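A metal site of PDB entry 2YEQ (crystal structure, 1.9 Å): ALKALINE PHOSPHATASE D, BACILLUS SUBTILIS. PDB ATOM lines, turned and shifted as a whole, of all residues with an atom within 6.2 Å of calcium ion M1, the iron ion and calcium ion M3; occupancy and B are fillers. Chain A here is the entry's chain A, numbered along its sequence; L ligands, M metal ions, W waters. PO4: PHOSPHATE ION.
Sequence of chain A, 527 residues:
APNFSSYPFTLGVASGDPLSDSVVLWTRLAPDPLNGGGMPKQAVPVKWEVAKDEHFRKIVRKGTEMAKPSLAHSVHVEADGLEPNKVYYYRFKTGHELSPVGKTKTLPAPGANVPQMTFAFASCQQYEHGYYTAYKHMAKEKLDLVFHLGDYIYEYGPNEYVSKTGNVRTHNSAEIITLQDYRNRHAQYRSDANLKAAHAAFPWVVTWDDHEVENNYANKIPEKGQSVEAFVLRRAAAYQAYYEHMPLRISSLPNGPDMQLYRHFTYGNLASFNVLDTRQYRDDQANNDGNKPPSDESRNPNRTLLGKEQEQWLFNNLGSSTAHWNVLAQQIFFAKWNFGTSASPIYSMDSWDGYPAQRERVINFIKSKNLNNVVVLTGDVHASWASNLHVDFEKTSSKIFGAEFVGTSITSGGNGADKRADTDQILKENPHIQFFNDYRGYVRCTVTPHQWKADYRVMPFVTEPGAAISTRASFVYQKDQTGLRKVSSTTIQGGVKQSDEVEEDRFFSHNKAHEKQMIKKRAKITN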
ATOM      1  N   SER A 123      -9.078  16.750   2.343  1.00  0.00           N
ATOM      2  CA  SER A 123      -9.615  17.686   3.346  1.00  0.00           C
ATOM      3  C   SER A 123      -9.902  16.925   4.610  1.00  0.00           C
ATOM      4  O   SER A 123      -9.946  15.696   4.610  1.00  0.00           O
ATOM      5  CB  SER A 123     -10.903  18.313   2.805  1.00  0.00           C
ATOM      6  OG  SER A 123     -11.916  17.341   2.702  1.00  0.00           O
ATOM      7  N   CYS A 124     -10.137  17.668   5.703  1.00  0.00           N
ATOM      8  CA  CYS A 124     -10.835  17.132   6.878  1.00  0.00           C
ATOM      9  C   CYS A 124     -10.115  15.976   7.603  1.00  0.00           C
ATOM     10  O   CYS A 124     -10.473  14.779   7.518  1.00  0.00           O
ATOM     11  CB  CYS A 124     -12.304  16.804   6.557  1.00  0.00           C
ATOM     12  SG  CYS A 124     -13.327  18.283   6.077  1.00  0.00           S
ATOM     13  N   GLN A 125      -9.132  16.377   8.397  1.00  0.00           N
ATOM     14  CA  GLN A 125      -8.247  15.425   9.055  1.00  0.00           C
ATOM     15  C   GLN A 125      -8.268  15.515  10.585  1.00  0.00           C
ATOM     16  O   GLN A 125      -7.211  15.576  11.209  1.00  0.00           O
ATOM     17  CB  GLN A 125      -6.825  15.582   8.508  1.00  0.00           C
ATOM     18  CG  GLN A 125      -6.219  16.965   8.597  1.00  0.00           C
ATOM     19  CD  GLN A 125      -5.133  17.175   7.610  1.00  0.00           C
ATOM     20  OE1 GLN A 125      -5.198  16.662   6.475  1.00  0.00           O
ATOM     21  NE2 GLN A 125      -4.122  17.963   7.983  1.00  0.00           N
ATOM     22  N   GLY A 150      -9.261  22.177   3.034  1.00  0.00           N
ATOM     23  CA  GLY A 150      -9.654  22.760   4.355  1.00  0.00           C
ATOM     24  C   GLY A 150      -9.787  21.757   5.482  1.00  0.00           C
ATOM     25  O   GLY A 150      -9.721  20.549   5.273  1.00  0.00           O
ATOM     26  N   ASP A 151     -10.028  22.306   6.685  1.00  0.00           N
ATOM     27  CA  ASP A 151     -10.052  21.569   7.916  1.00  0.00           C
ATOM     28  C   ASP A 151      -8.751  20.774   8.036  1.00  0.00           C
ATOM     29  O   ASP A 151      -8.763  19.599   8.387  1.00  0.00           O
ATOM     30  CB  ASP A 151     -11.287  20.693   8.046  1.00  0.00           C
ATOM     31  CG  ASP A 151     -12.592  21.488   8.156  1.00  0.00           C
ATOM     32  OD1 ASP A 151     -12.566  22.727   8.079  1.00  0.00           O
ATOM     33  OD2 ASP A 151     -13.663  20.823   8.278  1.00  0.00           O
ATOM     34  N   TYR A 154      -8.386  21.088  13.414  1.00  0.00           N
ATOM     35  CA  TYR A 154      -9.639  21.376  14.094  1.00  0.00           C
ATOM     36  C   TYR A 154      -9.259  22.078  15.413  1.00  0.00           C
ATOM     37  O   TYR A 154      -8.150  21.875  15.931  1.00  0.00           O
ATOM     38  CB  TYR A 154     -10.484  20.116  14.367  1.00  0.00           C
ATOM     39  CG  TYR A 154     -11.126  19.547  13.115  1.00  0.00           C
ATOM     40  CD1 TYR A 154     -10.349  18.964  12.102  1.00  0.00           C
ATOM     41  CD2 TYR A 154     -12.494  19.630  12.912  1.00  0.00           C
ATOM     42  CE1 TYR A 154     -10.916  18.472  10.937  1.00  0.00           C
ATOM     43  CE2 TYR A 154     -13.097  19.132  11.742  1.00  0.00           C
ATOM     44  CZ  TYR A 154     -12.298  18.567  10.759  1.00  0.00           C
ATOM     45  OH  TYR A 154     -12.858  18.058   9.622  1.00  0.00           O
ATOM     46  N   TYR A 161     -15.689  17.123  20.020  1.00  0.00           N
ATOM     47  CA  TYR A 161     -16.195  16.683  18.725  1.00  0.00           C
ATOM     48  C   TYR A 161     -15.840  15.212  18.569  1.00  0.00           C
ATOM     49  O   TYR A 161     -14.728  14.870  18.167  1.00  0.00           O
ATOM     50  CB  TYR A 161     -15.569  17.517  17.625  1.00  0.00           C
ATOM     51  CG  TYR A 161     -15.952  17.101  16.212  1.00  0.00           C
ATOM     52  CD1 TYR A 161     -17.163  16.474  15.925  1.00  0.00           C
ATOM     53  CD2 TYR A 161     -15.077  17.336  15.169  1.00  0.00           C
ATOM     54  CE1 TYR A 161     -17.484  16.101  14.648  1.00  0.00           C
ATOM     55  CE2 TYR A 161     -15.402  16.980  13.878  1.00  0.00           C
ATOM     56  CZ  TYR A 161     -16.599  16.366  13.623  1.00  0.00           C
ATOM     57  OH  TYR A 161     -16.888  15.981  12.338  1.00  0.00           O
ATOM     58  N   ASP A 209     -10.709  25.930   5.170  1.00  0.00           N
ATOM     59  CA  ASP A 209     -12.148  26.047   5.347  1.00  0.00           C
ATOM     60  C   ASP A 209     -12.382  26.624   6.761  1.00  0.00           C
ATOM     61  O   ASP A 209     -11.644  27.539   7.152  1.00  0.00           O
ATOM     62  CB  ASP A 209     -12.895  24.715   5.122  1.00  0.00           C
ATOM     63  CG  ASP A 209     -14.416  24.913   5.012  1.00  0.00           C
ATOM     64  OD1 ASP A 209     -14.868  25.952   4.439  1.00  0.00           O
ATOM     65  OD2 ASP A 209     -15.179  24.034   5.564  1.00  0.00           O
ATOM     66  N   ASP A 210     -13.335  26.106   7.516  1.00  0.00           N
ATOM     67  CA  ASP A 210     -13.715  26.774   8.787  1.00  0.00           C
ATOM     68  C   ASP A 210     -12.850  26.402   9.970  1.00  0.00           C
ATOM     69  O   ASP A 210     -12.519  27.271  10.777  1.00  0.00           O
ATOM     70  CB  ASP A 210     -15.200  26.580   9.168  1.00  0.00           C
ATOM     71  CG  ASP A 210     -15.672  25.154   9.092  1.00  0.00           C
ATOM     72  OD1 ASP A 210     -15.057  24.327   8.345  1.00  0.00           O
ATOM     73  OD2 ASP A 210     -16.687  24.825   9.751  1.00  0.00           O
ATOM     74  N   HIS A 211     -12.474  25.121  10.069  1.00  0.00           N
ATOM     75  CA  HIS A 211     -11.833  24.625  11.269  1.00  0.00           C
ATOM     76  C   HIS A 211     -10.394  25.055  11.478  1.00  0.00           C
ATOM     77  O   HIS A 211      -9.870  24.883  12.581  1.00  0.00           O
ATOM     78  CB  HIS A 211     -12.004  23.130  11.393  1.00  0.00           C
ATOM     79  CG  HIS A 211     -13.383  22.709  11.807  1.00  0.00           C
ATOM     80  ND1 HIS A 211     -13.872  22.923  13.082  1.00  0.00           N
ATOM     81  CD2 HIS A 211     -14.336  22.016  11.143  1.00  0.00           C
ATOM     82  CE1 HIS A 211     -15.080  22.369  13.175  1.00  0.00           C
ATOM     83  NE2 HIS A 211     -15.393  21.837  12.010  1.00  0.00           N
ATOM     84  N   ASN A 215     -15.373  26.367  13.890  1.00  0.00           N
ATOM     85  CA  ASN A 215     -16.530  25.815  13.172  1.00  0.00           C
ATOM     86  C   ASN A 215     -17.531  26.865  12.642  1.00  0.00           C
ATOM     87  O   ASN A 215     -18.044  27.702  13.418  1.00  0.00           O
ATOM     88  CB  ASN A 215     -17.316  24.846  14.057  1.00  0.00           C
ATOM     89  CG  ASN A 215     -18.348  24.048  13.263  1.00  0.00           C
ATOM     90  OD1 ASN A 215     -18.004  23.387  12.261  1.00  0.00           O
ATOM     91  ND2 ASN A 215     -19.607  24.082  13.714  1.00  0.00           N
ATOM     92  N   ASN A 216     -17.813  26.768  11.341  1.00  0.00           N
ATOM     93  CA  ASN A 216     -18.860  27.526  10.654  1.00  0.00           C
ATOM     94  C   ASN A 216     -18.783  29.025  10.800  1.00  0.00           C
ATOM     95  O   ASN A 216     -19.822  29.718  10.768  1.00  0.00           O
ATOM     96  CB  ASN A 216     -20.252  27.030  11.058  1.00  0.00           C
ATOM     97  CG  ASN A 216     -20.638  25.697  10.365  1.00  0.00           C
ATOM     98  OD1 ASN A 216     -19.801  24.829  10.203  1.00  0.00           O
ATOM     99  ND2 ASN A 216     -21.908  25.543   9.983  1.00  0.00           N
ATOM    100  N   ARG A 279     -14.614  31.299   2.931  1.00  0.00           N
ATOM    101  CA  ARG A 279     -14.813  31.644   4.339  1.00  0.00           C
ATOM    102  C   ARG A 279     -14.547  33.097   4.667  1.00  0.00           C
ATOM    103  O   ARG A 279     -15.316  33.685   5.435  1.00  0.00           O
ATOM    104  CB  ARG A 279     -13.890  30.825   5.263  1.00  0.00           C
ATOM    105  CG  ARG A 279     -14.336  29.434   5.474  1.00  0.00           C
ATOM    106  CD  ARG A 279     -15.592  29.280   6.237  1.00  0.00           C
ATOM    107  NE  ARG A 279     -16.090  27.916   6.094  1.00  0.00           N
ATOM    108  CZ  ARG A 279     -17.305  27.484   6.401  1.00  0.00           C
ATOM    109  NH1 ARG A 279     -18.237  28.300   6.954  1.00  0.00           N
ATOM    110  NH2 ARG A 279     -17.617  26.224   6.156  1.00  0.00           N
ATOM    111  N   GLN A 331     -14.088  24.723  -1.148  1.00  0.00           N
ATOM    112  CA  GLN A 331     -14.316  24.090   0.148  1.00  0.00           C
ATOM    113  C   GLN A 331     -15.554  23.261   0.293  1.00  0.00           C
ATOM    114  O   GLN A 331     -15.534  22.221   0.971  1.00  0.00           O
ATOM    115  CB  GLN A 331     -14.369  25.181   1.233  1.00  0.00           C
ATOM    116  CG  GLN A 331     -13.072  25.932   1.471  1.00  0.00           C
ATOM    117  CD  GLN A 331     -12.679  26.902   0.378  1.00  0.00           C
ATOM    118  OE1 GLN A 331     -13.514  27.418  -0.382  1.00  0.00           O
ATOM    119  NE2 GLN A 331     -11.369  27.195   0.304  1.00  0.00           N
ATOM    120  N   ILE A 332     -16.666  23.758  -0.260  1.00  0.00           N
ATOM    121  CA  ILE A 332     -17.974  23.313   0.164  1.00  0.00           C
ATOM    122  C   ILE A 332     -18.867  22.814  -1.009  1.00  0.00           C
ATOM    123  O   ILE A 332     -18.640  23.110  -2.173  1.00  0.00           O
ATOM    124  CB  ILE A 332     -18.715  24.455   0.934  1.00  0.00           C
ATOM    125  CG1 ILE A 332     -18.610  25.768   0.177  1.00  0.00           C
ATOM    126  CG2 ILE A 332     -18.144  24.608   2.399  1.00  0.00           C
ATOM    127  CD1 ILE A 332     -19.640  26.831   0.606  1.00  0.00           C
ATOM    128  N   ASP A 350     -24.742  26.157   5.047  1.00  0.00           N
ATOM    129  CA  ASP A 350     -23.289  26.442   5.012  1.00  0.00           C
ATOM    130  C   ASP A 350     -22.613  26.113   3.677  1.00  0.00           C
ATOM    131  O   ASP A 350     -21.466  26.491   3.435  1.00  0.00           O
ATOM    132  CB  ASP A 350     -22.614  25.673   6.148  1.00  0.00           C
ATOM    133  CG  ASP A 350     -21.180  26.121   6.381  1.00  0.00           C
ATOM    134  OD1 ASP A 350     -20.920  27.334   6.597  1.00  0.00           O
ATOM    135  OD2 ASP A 350     -20.298  25.215   6.361  1.00  0.00           O
ATOM    136  N   ASP A 380     -15.229  19.222   2.983  1.00  0.00           N
ATOM    137  CA  ASP A 380     -16.191  19.670   4.031  1.00  0.00           C
ATOM    138  C   ASP A 380     -17.178  18.643   4.541  1.00  0.00           C
ATOM    139  O   ASP A 380     -17.428  18.580   5.751  1.00  0.00           O
ATOM    140  CB  ASP A 380     -16.902  20.978   3.639  1.00  0.00           C
ATOM    141  CG  ASP A 380     -17.791  21.525   4.782  1.00  0.00           C
ATOM    142  OD1 ASP A 380     -17.249  21.970   5.837  1.00  0.00           O
ATOM    143  OD2 ASP A 380     -19.039  21.451   4.612  1.00  0.00           O
ATOM    144  N   VAL A 381     -17.699  17.810   3.649  1.00  0.00           N
ATOM    145  CA  VAL A 381     -18.854  16.984   3.991  1.00  0.00           C
ATOM    146  C   VAL A 381     -18.532  15.593   4.484  1.00  0.00           C
ATOM    147  O   VAL A 381     -19.417  14.844   4.855  1.00  0.00           O
ATOM    148  CB  VAL A 381     -19.923  16.951   2.817  1.00  0.00           C
ATOM    149  CG1 VAL A 381     -20.268  18.402   2.388  1.00  0.00           C
ATOM    150  CG2 VAL A 381     -19.450  16.081   1.633  1.00  0.00           C
ATOM    151  N   HIS A 382     -17.245  15.266   4.561  1.00  0.00           N
ATOM    152  CA  HIS A 382     -16.780  14.032   5.223  1.00  0.00           C
ATOM    153  C   HIS A 382     -17.324  12.754   4.553  1.00  0.00           C
ATOM    154  O   HIS A 382     -17.570  11.752   5.191  1.00  0.00           O
ATOM    155  CB  HIS A 382     -17.122  14.030   6.724  1.00  0.00           C
ATOM    156  CG  HIS A 382     -16.546  15.200   7.498  1.00  0.00           C
ATOM    157  ND1 HIS A 382     -16.885  15.418   8.817  1.00  0.00           N
ATOM    158  CD2 HIS A 382     -15.688  16.181   7.159  1.00  0.00           C
ATOM    159  CE1 HIS A 382     -16.259  16.498   9.260  1.00  0.00           C
ATOM    160  NE2 HIS A 382     -15.521  16.992   8.281  1.00  0.00           N
ATOM    161  N   SER A 409     -13.318  12.732   3.759  1.00  0.00           N
ATOM    162  CA  SER A 409     -12.344  13.235   4.716  1.00  0.00           C
ATOM    163  C   SER A 409     -11.186  12.225   4.904  1.00  0.00           C
ATOM    164  O   SER A 409     -11.382  11.018   4.749  1.00  0.00           O
ATOM    165  CB  SER A 409     -13.052  13.419   6.026  1.00  0.00           C
ATOM    166  OG  SER A 409     -13.825  12.281   6.364  1.00  0.00           O
ATOM    167  N   SER A 412     -12.023  12.724   9.460  1.00  0.00           N
ATOM    168  CA  SER A 412     -13.169  13.273  10.221  1.00  0.00           C
ATOM    169  C   SER A 412     -14.371  12.388  10.032  1.00  0.00           C
ATOM    170  O   SER A 412     -14.712  12.020   8.901  1.00  0.00           O
ATOM    171  CB  SER A 412     -13.502  14.700   9.775  1.00  0.00           C
ATOM    172  OG  SER A 412     -12.360  15.507   9.843  1.00  0.00           O
ATOM    173  N   ARG A 506     -23.569  15.062  11.217  1.00  0.00           N
ATOM    174  CA  ARG A 506     -22.421  15.954  11.209  1.00  0.00           C
ATOM    175  C   ARG A 506     -22.743  17.289  11.940  1.00  0.00           C
ATOM    176  O   ARG A 506     -21.986  17.719  12.800  1.00  0.00           O
ATOM    177  CB  ARG A 506     -21.926  16.180   9.776  1.00  0.00           C
ATOM    178  CG  ARG A 506     -20.642  16.992   9.655  1.00  0.00           C
ATOM    179  CD  ARG A 506     -20.060  16.917   8.268  1.00  0.00           C
ATOM    180  NE  ARG A 506     -21.015  17.365   7.251  1.00  0.00           N
ATOM    181  CZ  ARG A 506     -21.043  18.570   6.675  1.00  0.00           C
ATOM    182  NH1 ARG A 506     -20.148  19.520   6.960  1.00  0.00           N
ATOM    183  NH2 ARG A 506     -21.990  18.818   5.761  1.00  0.00           N
ATOM    184  N   HIS A 510     -21.207  18.373  15.713  1.00  0.00           N
ATOM    185  CA  HIS A 510     -20.583  19.673  15.961  1.00  0.00           C
ATOM    186  C   HIS A 510     -21.335  20.500  17.036  1.00  0.00           C
ATOM    187  O   HIS A 510     -20.702  21.263  17.763  1.00  0.00           O
ATOM    188  CB  HIS A 510     -20.509  20.477  14.677  1.00  0.00           C
ATOM    189  CG  HIS A 510     -19.449  20.024  13.733  1.00  0.00           C
ATOM    190  ND1 HIS A 510     -19.611  18.949  12.881  1.00  0.00           N
ATOM    191  CD2 HIS A 510     -18.211  20.504  13.485  1.00  0.00           C
ATOM    192  CE1 HIS A 510     -18.533  18.795  12.146  1.00  0.00           C
ATOM    193  NE2 HIS A 510     -17.665  19.736  12.484  1.00  0.00           N
HETATM  194  P   PO4 L   1     -16.750  20.144   8.941  1.00  0.00           P
HETATM  195  O1  PO4 L   1     -18.138  19.638   8.969  1.00  0.00           O
HETATM  196  O2  PO4 L   1     -16.570  21.630   8.903  1.00  0.00           O
HETATM  197  O3  PO4 L   1     -15.853  19.401   9.916  1.00  0.00           O
HETATM  198  O4  PO4 L   1     -16.136  19.855   7.535  1.00  0.00           O
HETATM  199 CA    CA M   1     -15.296  22.330   7.106  1.00  0.00          CA
HETATM  200 FE    FE M   2     -14.247  18.750   8.365  1.00  0.00          FE
HETATM  201 CA    CA M   3     -18.198  23.123   9.927  1.00  0.00          CA
HETATM  202  O   HOH W   1     -13.688  21.350   5.348  1.00  0.00           O
HETATM  203  O   HOH W   2     -18.762  23.319   7.642  1.00  0.00           O
HETATM  204  O   HOH W   3     -19.637  21.447  10.229  1.00  0.00           O
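The side-chain sulfur of Cys 124 lies close to the backbone NH of Asp 380 (3.8 Å).
SG of Cys 124 sits close to OG of Ser 123 (3.8 Å).
NE of Arg 279 is in salt-bridge range of OD1 of Asp 209 (2.8 Å).
A ring nitrogen (NE2) of His 211 sits close to the side-chain amide oxygen (OD1) of Asn 215 (3.0 Å).
OD1 of Asp 210 lies close to NH2 of Arg 279 (3.9 Å).
The backbone carbonyl oxygen (O) of Gly 150 lies within hydrogen-bond range of the backbone NH (N) of Cys 124.
The backbone carbonyl oxygen of Asp 151 is in hydrogen-bond range of the backbone NH of Gln 125 (3.2 Å).
The side-chain carboxylate of Asp 380 lies within salt-bridge range of the guanidinium group of Arg 506.
The nearest printed residue that does not touch calcium ion M1 is His 211 (4.2 Å).
Merely in contact with calcium ion M3: His 211 (3.7 Å).
Within 4 Å of calcium ion M3: Asp 210, His 211, Asn 215 and Asn 216.
Along chain A the residues within 4 Å of calcium ion M3 span positions 210 to 216.
The nearest printed residue that does not touch calcium ion M3 is His 510 (4.3 Å).
Calcium ion M1 is bound by OD2 of Asp 209 (2.3 Å), O2 of the ligand (2.3 Å), OD1 of Asp 380 (2.4 Å), OD1 of Asp 210 (2.4 Å), OD2 of Asp 151 (2.5 Å), water W1 (2.6 Å) and O4 of the ligand (2.6 Å).
Calcium ion M1 has seven donor atoms within binding distance.
Slightly farther from calcium ion M1 lies OD1 of Asp 151 (2.9 Å).
The iron ion is bound by OH of Tyr 154 (2.0 Å), OD2 of Asp 151 (2.2 Å), NE2 of His 382 (2.2 Å), O3 of the ligand (2.3 Å), O4 of the ligand (2.3 Å) and SG of Cys 124 (2.5 Å).
The iron ion has six donor atoms within binding distance.
Calcium ion M3 is bound by water W3 (2.2 Å), the side-chain carboxylate of Asp 210 (2.3 Å), the side-chain amide oxygen of Asn 215 (2.4 Å), the side-chain amide oxygen of Asn 216 (2.4 Å), water W2 (2.4 Å) and an oxygen (O2) of the ligand (2.4 Å).
Water W2 bridges the side-chain carboxylate (OD2) of Asp 350 (2.8 Å) and the guanidinium group (NH2) of Arg 279 (3.5 Å).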
